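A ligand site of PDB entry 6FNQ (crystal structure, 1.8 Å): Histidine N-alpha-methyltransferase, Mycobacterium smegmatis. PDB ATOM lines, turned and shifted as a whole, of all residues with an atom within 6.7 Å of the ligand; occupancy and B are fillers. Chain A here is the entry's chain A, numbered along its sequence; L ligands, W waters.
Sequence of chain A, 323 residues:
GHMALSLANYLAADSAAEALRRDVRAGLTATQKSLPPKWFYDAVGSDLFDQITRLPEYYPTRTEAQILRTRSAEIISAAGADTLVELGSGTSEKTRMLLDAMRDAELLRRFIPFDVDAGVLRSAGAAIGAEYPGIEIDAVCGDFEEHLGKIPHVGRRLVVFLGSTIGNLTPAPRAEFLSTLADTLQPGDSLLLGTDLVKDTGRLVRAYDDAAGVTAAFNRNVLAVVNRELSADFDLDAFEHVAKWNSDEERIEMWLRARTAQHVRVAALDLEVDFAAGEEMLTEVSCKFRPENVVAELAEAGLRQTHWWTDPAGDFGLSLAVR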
ATOM      1  N   PHE A  40       7.005 -11.750 -37.758  1.00  0.00           N
ATOM      2  CA  PHE A  40       6.795 -12.414 -36.484  1.00  0.00           C
ATOM      3  C   PHE A  40       5.306 -12.524 -36.163  1.00  0.00           C
ATOM      4  O   PHE A  40       4.893 -13.395 -35.394  1.00  0.00           O
ATOM      5  CB  PHE A  40       7.432 -11.642 -35.308  1.00  0.00           C
ATOM      6  CG  PHE A  40       8.918 -11.762 -35.173  1.00  0.00           C
ATOM      7  CD1 PHE A  40       9.560 -12.987 -35.261  1.00  0.00           C
ATOM      8  CD2 PHE A  40       9.660 -10.645 -34.842  1.00  0.00           C
ATOM      9  CE1 PHE A  40      10.935 -13.062 -35.102  1.00  0.00           C
ATOM     10  CE2 PHE A  40      11.044 -10.724 -34.663  1.00  0.00           C
ATOM     11  CZ  PHE A  40      11.659 -11.931 -34.780  1.00  0.00           C
ATOM     12  N   TYR A  41       4.486 -11.603 -36.680  1.00  0.00           N
ATOM     13  CA  TYR A  41       3.168 -11.350 -36.089  1.00  0.00           C
ATOM     14  C   TYR A  41       2.046 -12.015 -36.878  1.00  0.00           C
ATOM     15  O   TYR A  41       1.014 -11.425 -37.179  1.00  0.00           O
ATOM     16  CB  TYR A  41       2.964  -9.831 -35.954  1.00  0.00           C
ATOM     17  CG  TYR A  41       4.011  -9.191 -35.065  1.00  0.00           C
ATOM     18  CD1 TYR A  41       3.895  -9.228 -33.673  1.00  0.00           C
ATOM     19  CD2 TYR A  41       5.146  -8.606 -35.608  1.00  0.00           C
ATOM     20  CE1 TYR A  41       4.880  -8.685 -32.854  1.00  0.00           C
ATOM     21  CE2 TYR A  41       6.117  -8.016 -34.798  1.00  0.00           C
ATOM     22  CZ  TYR A  41       5.970  -8.056 -33.428  1.00  0.00           C
ATOM     23  OH  TYR A  41       6.952  -7.486 -32.628  1.00  0.00           O
ATOM     24  N   PHE A  49       3.838 -12.657 -28.477  1.00  0.00           N
ATOM     25  CA  PHE A  49       4.216 -11.302 -28.094  1.00  0.00           C
ATOM     26  C   PHE A  49       3.345 -10.789 -26.942  1.00  0.00           C
ATOM     27  O   PHE A  49       3.843 -10.141 -26.012  1.00  0.00           O
ATOM     28  CB  PHE A  49       4.134 -10.310 -29.248  1.00  0.00           C
ATOM     29  CG  PHE A  49       4.443  -8.896 -28.783  1.00  0.00           C
ATOM     30  CD1 PHE A  49       5.692  -8.568 -28.329  1.00  0.00           C
ATOM     31  CD2 PHE A  49       3.424  -7.971 -28.651  1.00  0.00           C
ATOM     32  CE1 PHE A  49       5.961  -7.316 -27.812  1.00  0.00           C
ATOM     33  CE2 PHE A  49       3.680  -6.724 -28.139  1.00  0.00           C
ATOM     34  CZ  PHE A  49       4.935  -6.391 -27.723  1.00  0.00           C
ATOM     35  N   ILE A  52       4.858 -12.073 -23.967  1.00  0.00           N
ATOM     36  CA  ILE A  52       6.105 -11.382 -23.667  1.00  0.00           C
ATOM     37  C   ILE A  52       5.838 -10.140 -22.844  1.00  0.00           C
ATOM     38  O   ILE A  52       6.598  -9.815 -21.915  1.00  0.00           O
ATOM     39  CB  ILE A  52       6.856 -11.013 -24.969  1.00  0.00           C
ATOM     40  CG1 ILE A  52       7.525 -12.281 -25.581  1.00  0.00           C
ATOM     41  CG2 ILE A  52       7.950  -9.973 -24.713  1.00  0.00           C
ATOM     42  CD1 ILE A  52       8.048 -12.080 -26.942  1.00  0.00           C
ATOM     43  N   TYR A  58      10.652  -8.418 -19.225  1.00  0.00           N
ATOM     44  CA  TYR A  58      10.290  -7.484 -20.287  1.00  0.00           C
ATOM     45  C   TYR A  58       9.584  -6.279 -19.666  1.00  0.00           C
ATOM     46  O   TYR A  58       8.341  -6.147 -19.634  1.00  0.00           O
ATOM     47  CB  TYR A  58       9.419  -8.164 -21.334  1.00  0.00           C
ATOM     48  CG  TYR A  58       9.218  -7.320 -22.566  1.00  0.00           C
ATOM     49  CD1 TYR A  58      10.240  -7.172 -23.520  1.00  0.00           C
ATOM     50  CD2 TYR A  58       8.026  -6.610 -22.761  1.00  0.00           C
ATOM     51  CE1 TYR A  58      10.072  -6.370 -24.641  1.00  0.00           C
ATOM     52  CE2 TYR A  58       7.858  -5.803 -23.906  1.00  0.00           C
ATOM     53  CZ  TYR A  58       8.873  -5.701 -24.821  1.00  0.00           C
ATOM     54  OH  TYR A  58       8.681  -4.891 -25.915  1.00  0.00           O
ATOM     55  N   PRO A  60       9.358  -3.086 -20.725  1.00  0.00           N
ATOM     56  CA  PRO A  60       8.775  -1.929 -21.450  1.00  0.00           C
ATOM     57  C   PRO A  60       7.264  -1.754 -21.319  1.00  0.00           C
ATOM     58  O   PRO A  60       6.790  -0.630 -21.093  1.00  0.00           O
ATOM     59  CB  PRO A  60       9.180  -2.193 -22.926  1.00  0.00           C
ATOM     60  CG  PRO A  60      10.419  -2.963 -22.839  1.00  0.00           C
ATOM     61  CD  PRO A  60      10.322  -3.827 -21.564  1.00  0.00           C
ATOM     62  N   LEU A 162       3.078   3.793 -29.617  1.00  0.00           N
ATOM     63  CA  LEU A 162       3.601   3.380 -28.329  1.00  0.00           C
ATOM     64  C   LEU A 162       4.499   2.143 -28.445  1.00  0.00           C
ATOM     65  O   LEU A 162       4.670   1.546 -29.520  1.00  0.00           O
ATOM     66  CB  LEU A 162       2.427   3.120 -27.377  1.00  0.00           C
ATOM     67  CG  LEU A 162       1.450   4.286 -27.278  1.00  0.00           C
ATOM     68  CD1 LEU A 162       0.271   3.865 -26.374  1.00  0.00           C
ATOM     69  CD2 LEU A 162       2.116   5.532 -26.763  1.00  0.00           C
ATOM     70  N   GLY A 163       5.086   1.763 -27.309  1.00  0.00           N
ATOM     71  CA  GLY A 163       5.758   0.481 -27.192  1.00  0.00           C
ATOM     72  C   GLY A 163       7.200   0.453 -27.652  1.00  0.00           C
ATOM     73  O   GLY A 163       7.863  -0.597 -27.536  1.00  0.00           O
ATOM     74  N   SER A 164       7.711   1.579 -28.147  1.00  0.00           N
ATOM     75  CA  SER A 164       9.033   1.635 -28.746  1.00  0.00           C
ATOM     76  C   SER A 164       9.118   0.800 -30.027  1.00  0.00           C
ATOM     77  O   SER A 164      10.200   0.434 -30.449  1.00  0.00           O
ATOM     78  CB  SER A 164      10.136   1.212 -27.773  1.00  0.00           C
ATOM     79  OG  SER A 164      11.385   1.875 -28.103  1.00  0.00           O
ATOM     80  N   THR A 165       7.984   0.592 -30.699  1.00  0.00           N
ATOM     81  CA  THR A 165       8.009  -0.016 -32.028  1.00  0.00           C
ATOM     82  C   THR A 165       8.795   0.833 -33.005  1.00  0.00           C
ATOM     83  O   THR A 165       9.344   0.297 -33.986  1.00  0.00           O
ATOM     84  CB  THR A 165       6.574  -0.259 -32.510  1.00  0.00           C
ATOM     85  OG1 THR A 165       5.976  -1.191 -31.605  1.00  0.00           O
ATOM     86  CG2 THR A 165       6.538  -0.843 -33.893  1.00  0.00           C
ATOM     87  N   ILE A 166       8.912   2.135 -32.749  1.00  0.00           N
ATOM     88  CA  ILE A 166       9.746   2.955 -33.623  1.00  0.00           C
ATOM     89  C   ILE A 166      11.182   2.455 -33.608  1.00  0.00           C
ATOM     90  O   ILE A 166      11.920   2.639 -34.586  1.00  0.00           O
ATOM     91  CB  ILE A 166       9.673   4.442 -33.215  1.00  0.00           C
ATOM     92  CG1 ILE A 166      10.269   5.306 -34.352  1.00  0.00           C
ATOM     93  CG2 ILE A 166      10.340   4.666 -31.895  1.00  0.00           C
ATOM     94  CD1 ILE A 166      10.031   6.729 -34.220  1.00  0.00           C
ATOM     95  N   GLY A 167      11.620   1.804 -32.526  1.00  0.00           N
ATOM     96  CA  GLY A 167      12.979   1.260 -32.450  1.00  0.00           C
ATOM     97  C   GLY A 167      13.274   0.126 -33.414  1.00  0.00           C
ATOM     98  O   GLY A 167      14.423  -0.287 -33.537  1.00  0.00           O
ATOM     99  N   ASN A 168      12.245  -0.408 -34.067  1.00  0.00           N
ATOM    100  CA  ASN A 168      12.483  -1.442 -35.086  1.00  0.00           C
ATOM    101  C   ASN A 168      13.008  -0.844 -36.382  1.00  0.00           C
ATOM    102  O   ASN A 168      13.504  -1.577 -37.251  1.00  0.00           O
ATOM    103  CB  ASN A 168      11.199  -2.209 -35.438  1.00  0.00           C
ATOM    104  CG  ASN A 168      10.787  -3.275 -34.424  1.00  0.00           C
ATOM    105  OD1 ASN A 168       9.607  -3.631 -34.375  1.00  0.00           O
ATOM    106  ND2 ASN A 168      11.729  -3.795 -33.630  1.00  0.00           N
ATOM    107  N   ASP A 196      11.898   3.340 -25.766  1.00  0.00           N
ATOM    108  CA  ASP A 196      12.679   2.671 -24.719  1.00  0.00           C
ATOM    109  C   ASP A 196      14.086   3.247 -24.658  1.00  0.00           C
ATOM    110  O   ASP A 196      14.667   3.608 -25.681  1.00  0.00           O
ATOM    111  CB  ASP A 196      12.717   1.171 -24.978  1.00  0.00           C
ATOM    112  CG  ASP A 196      13.175   0.371 -23.770  1.00  0.00           C
ATOM    113  OD1 ASP A 196      13.248   0.946 -22.650  1.00  0.00           O
ATOM    114  OD2 ASP A 196      13.449  -0.835 -23.936  1.00  0.00           O
ATOM    115  N   ALA A 207      15.704  -8.723 -21.083  1.00  0.00           N
ATOM    116  CA  ALA A 207      14.369  -8.403 -21.573  1.00  0.00           C
ATOM    117  C   ALA A 207      14.061  -9.092 -22.896  1.00  0.00           C
ATOM    118  O   ALA A 207      12.875  -9.262 -23.243  1.00  0.00           O
ATOM    119  CB  ALA A 207      14.209  -6.899 -21.745  1.00  0.00           C
ATOM    120  N   TYR A 208      15.099  -9.504 -23.641  1.00  0.00           N
ATOM    121  CA  TYR A 208      14.954 -10.167 -24.929  1.00  0.00           C
ATOM    122  C   TYR A 208      15.479 -11.610 -24.911  1.00  0.00           C
ATOM    123  O   TYR A 208      15.665 -12.205 -25.947  1.00  0.00           O
ATOM    124  CB  TYR A 208      15.667  -9.341 -26.016  1.00  0.00           C
ATOM    125  CG  TYR A 208      14.971  -8.010 -26.218  1.00  0.00           C
ATOM    126  CD1 TYR A 208      15.196  -6.945 -25.343  1.00  0.00           C
ATOM    127  CD2 TYR A 208      14.045  -7.829 -27.243  1.00  0.00           C
ATOM    128  CE1 TYR A 208      14.535  -5.750 -25.482  1.00  0.00           C
ATOM    129  CE2 TYR A 208      13.380  -6.624 -27.384  1.00  0.00           C
ATOM    130  CZ  TYR A 208      13.627  -5.583 -26.498  1.00  0.00           C
ATOM    131  OH  TYR A 208      12.951  -4.365 -26.606  1.00  0.00           O
ATOM    132  N   THR A 215      10.558 -15.586 -25.389  1.00  0.00           N
ATOM    133  CA  THR A 215      11.108 -14.792 -26.488  1.00  0.00           C
ATOM    134  C   THR A 215      11.782 -15.684 -27.523  1.00  0.00           C
ATOM    135  O   THR A 215      11.642 -15.456 -28.733  1.00  0.00           O
ATOM    136  CB  THR A 215      12.082 -13.756 -25.959  1.00  0.00           C
ATOM    137  OG1 THR A 215      11.443 -12.929 -24.981  1.00  0.00           O
ATOM    138  CG2 THR A 215      12.566 -12.901 -27.076  1.00  0.00           C
ATOM    139  N   PHE A 218       9.034 -17.032 -29.695  1.00  0.00           N
ATOM    140  CA  PHE A 218       8.614 -15.951 -30.574  1.00  0.00           C
ATOM    141  C   PHE A 218       9.575 -15.779 -31.745  1.00  0.00           C
ATOM    142  O   PHE A 218       9.148 -15.639 -32.896  1.00  0.00           O
ATOM    143  CB  PHE A 218       8.532 -14.658 -29.730  1.00  0.00           C
ATOM    144  CG  PHE A 218       8.239 -13.411 -30.504  1.00  0.00           C
ATOM    145  CD1 PHE A 218       6.952 -13.156 -30.968  1.00  0.00           C
ATOM    146  CD2 PHE A 218       9.217 -12.449 -30.680  1.00  0.00           C
ATOM    147  CE1 PHE A 218       6.682 -11.977 -31.642  1.00  0.00           C
ATOM    148  CE2 PHE A 218       8.951 -11.280 -31.351  1.00  0.00           C
ATOM    149  CZ  PHE A 218       7.654 -11.040 -31.819  1.00  0.00           C
ATOM    150  N   ILE A 252      19.330  -3.345 -29.231  1.00  0.00           N
ATOM    151  CA  ILE A 252      19.211  -4.787 -29.005  1.00  0.00           C
ATOM    152  C   ILE A 252      19.060  -5.443 -30.359  1.00  0.00           C
ATOM    153  O   ILE A 252      18.477  -4.861 -31.294  1.00  0.00           O
ATOM    154  CB  ILE A 252      18.015  -5.090 -28.077  1.00  0.00           C
ATOM    155  CG1 ILE A 252      18.432  -4.891 -26.598  1.00  0.00           C
ATOM    156  CG2 ILE A 252      17.417  -6.467 -28.389  1.00  0.00           C
ATOM    157  CD1 ILE A 252      19.430  -5.924 -26.062  1.00  0.00           C
ATOM    158  N   MET A 254      18.043  -9.429 -32.043  1.00  0.00           N
ATOM    159  CA  MET A 254      17.692 -10.838 -31.934  1.00  0.00           C
ATOM    160  C   MET A 254      18.264 -11.563 -33.151  1.00  0.00           C
ATOM    161  O   MET A 254      18.158 -11.077 -34.296  1.00  0.00           O
ATOM    162  CB  MET A 254      16.197 -11.067 -31.828  1.00  0.00           C
ATOM    163  CG  MET A 254      15.547 -10.464 -30.570  1.00  0.00           C
ATOM    164  SD  MET A 254      14.056 -11.301 -30.039  1.00  0.00           S
ATOM    165  CE  MET A 254      13.202 -11.464 -31.567  1.00  0.00           C
ATOM    166  N   GLU A 284      15.719  -9.239 -35.773  1.00  0.00           N
ATOM    167  CA  GLU A 284      15.097  -8.025 -35.238  1.00  0.00           C
ATOM    168  C   GLU A 284      16.176  -7.100 -34.677  1.00  0.00           C
ATOM    169  O   GLU A 284      17.135  -7.562 -34.050  1.00  0.00           O
ATOM    170  CB  GLU A 284      14.089  -8.341 -34.128  1.00  0.00           C
ATOM    171  CG  GLU A 284      13.253  -7.133 -33.716  1.00  0.00           C
ATOM    172  CD  GLU A 284      12.212  -7.400 -32.631  1.00  0.00           C
ATOM    173  OE1 GLU A 284      12.401  -8.333 -31.829  1.00  0.00           O
ATOM    174  OE2 GLU A 284      11.208  -6.660 -32.592  1.00  0.00           O
ATOM    175  N   VAL A 285      16.010  -5.799 -34.896  1.00  0.00           N
ATOM    176  CA  VAL A 285      16.729  -4.792 -34.117  1.00  0.00           C
ATOM    177  C   VAL A 285      15.718  -3.997 -33.311  1.00  0.00           C
ATOM    178  O   VAL A 285      14.569  -3.775 -33.724  1.00  0.00           O
ATOM    179  CB  VAL A 285      17.589  -3.847 -34.994  1.00  0.00           C
ATOM    180  CG1 VAL A 285      18.539  -4.654 -35.875  1.00  0.00           C
ATOM    181  CG2 VAL A 285      16.733  -2.933 -35.816  1.00  0.00           C
ATOM    182  N   SER A 286      16.151  -3.574 -32.125  1.00  0.00           N
ATOM    183  CA  SER A 286      15.297  -2.776 -31.230  1.00  0.00           C
ATOM    184  C   SER A 286      16.188  -1.659 -30.698  1.00  0.00           C
ATOM    185  O   SER A 286      16.921  -1.844 -29.715  1.00  0.00           O
ATOM    186  CB  SER A 286      14.690  -3.622 -30.139  1.00  0.00           C
ATOM    187  OG  SER A 286      13.720  -2.874 -29.421  1.00  0.00           O
ATOM    188  N   CYS A 287      16.160  -0.518 -31.398  1.00  0.00           N
ATOM    189  CA  CYS A 287      17.020   0.608 -31.044  1.00  0.00           C
ATOM    190  C   CYS A 287      16.573   1.211 -29.723  1.00  0.00           C
ATOM    191  O   CYS A 287      15.378   1.286 -29.416  1.00  0.00           O
ATOM    192  CB  CYS A 287      16.993   1.643 -32.174  1.00  0.00           C
ATOM    193  SG  CYS A 287      17.646   1.026 -33.836  1.00  0.00           S
ATOM    194  N   LYS A 288      17.538   1.599 -28.905  1.00  0.00           N
ATOM    195  CA  LYS A 288      17.284   2.194 -27.604  1.00  0.00           C
ATOM    196  C   LYS A 288      17.819   3.611 -27.635  1.00  0.00           C
ATOM    197  O   LYS A 288      18.808   3.917 -28.339  1.00  0.00           O
ATOM    198  CB  LYS A 288      17.928   1.385 -26.511  1.00  0.00           C
ATOM    199  CG  LYS A 288      17.503  -0.089 -26.456  1.00  0.00           C
ATOM    200  CD  LYS A 288      15.992  -0.231 -26.261  1.00  0.00           C
ATOM    201  CE  LYS A 288      15.560  -1.676 -26.476  1.00  0.00           C
ATOM    202  NZ  LYS A 288      14.077  -1.841 -26.438  1.00  0.00           N
HETATM  203  C1  LIG L   1       8.688  -4.124 -31.450  1.00  0.00           C
HETATM  204  C2  LIG L   1       6.805  -4.560 -30.115  1.00  0.00           C
HETATM  205  C3  LIG L   1       8.319  -2.888 -29.479  1.00  0.00           C
HETATM  206  O1  LIG L   1      10.590  -4.618 -27.627  1.00  0.00           O
HETATM  207  O2  LIG L   1      11.249  -4.345 -29.693  1.00  0.00           O
HETATM  208  C4  LIG L   1       9.728  -7.962 -27.876  1.00  0.00           C
HETATM  209  C5  LIG L   1       9.143  -6.532 -30.014  1.00  0.00           C
HETATM  210  N1  LIG L   1      10.903  -8.401 -29.726  1.00  0.00           N
HETATM  211  N2  LIG L   1      10.606  -8.994 -27.576  1.00  0.00           N
HETATM  212  C6  LIG L   1      10.365  -4.718 -28.850  1.00  0.00           C
HETATM  213  C7  LIG L   1       9.909  -7.604 -29.201  1.00  0.00           C
HETATM  214  C8  LIG L   1      11.330  -9.248 -28.701  1.00  0.00           C
HETATM  215  C9  LIG L   1       8.991  -5.187 -29.283  1.00  0.00           C
HETATM  216  N3  LIG L   1       8.230  -4.195 -30.074  1.00  0.00           N
HETATM  217  O   HOH W   1      11.989  -1.399 -30.611  1.00  0.00           O
HETATM  218  O   HOH W   2      11.377 -10.305 -25.296  1.00  0.00           O
HETATM  219  O   HOH W   3       9.039  -6.425 -33.925  1.00  0.00           O
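The side-chain amide nitrogen (ND2) of Asn 168 lies within hydrogen-bond range of the side-chain carboxylate (OE2) of Glu 284 (3.1 Å). The backbone NH of Met 254 is in hydrogen-bond range of the backbone carbonyl oxygen of Glu 284 (2.9 Å). The side-chain hydroxyl (OG) of Ser 286 is in hydrogen-bond range of the side-chain hydroxyl (OH) of Tyr 208 (3.3 Å). OH of Tyr 208 sits at hydrogen-bond distance from NZ of Lys 288 (2.8 Å). The side-chain hydroxyl (OG) of Ser 286 sits at hydrogen-bond distance from the side-chain amino group (NZ) of Lys 288. N of Ser 286 lies within hydrogen-bond range of O of Ile 252 (2.8 Å). The side-chain amide nitrogen (ND2) of Asn 168 sits at hydrogen-bond distance from the backbone carbonyl oxygen (O) of Val 285 (2.8 Å). The side-chain hydroxyl of Ser 164 sits at hydrogen-bond distance from the backbone NH of Asp 196 (2.8 Å).
O1 of the ligand lies within hydrogen-bond range of OH of Tyr 58, at 2.6 Å. The side-chain carboxylate (OE1) of Glu 284 is in hydrogen-bond range of a nitrogen (N1) of the ligand, at 2.6 Å. OH of Tyr 208 is in hydrogen-bond range of O1 of the ligand, at 2.6 Å. The side-chain hydroxyl (OG) of Ser 286 sits at hydrogen-bond distance from an oxygen (O2) of the ligand (2.9 Å).
Merely in contact with the ligand: Gly 163 (3.0 Å), Asn 168 (3.1 Å), Tyr 41 (3.5 Å), Phe 49 (3.5 Å), Thr 165 (3.6 Å), Met 254 (3.7 Å), Ser 164 (3.8 Å) and Phe 218 (3.8 Å). Hydrophobic or aromatic side chains that line the ligand: Phe 49, Tyr 58, Tyr 208, Phe 218 and Met 254. Within 4 Å of the ligand: Tyr 41, Phe 49, Tyr 58, Gly 163, Ser 164, Thr 165, Asn 168, Tyr 208, Phe 218, Met 254, Glu 284 and Ser 286.
Water W2 lies within hydrogen-bond range of OG1 of Thr 215 (2.6 Å), N2 of the ligand (2.7 Å) and O of Ala 207 (2.7 Å). Water W1 lies within hydrogen-bond range of the backbone carbonyl oxygen of Ser 164, the side-chain hydroxyl of Ser 286 and an oxygen (O2) of the ligand. Water W3 lies within hydrogen-bond range of the side-chain carboxylate of Glu 284 (2.6 Å), the side-chain hydroxyl of Tyr 41 (2.7 Å) and the side-chain amide oxygen of Asn 168 (2.9 Å).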
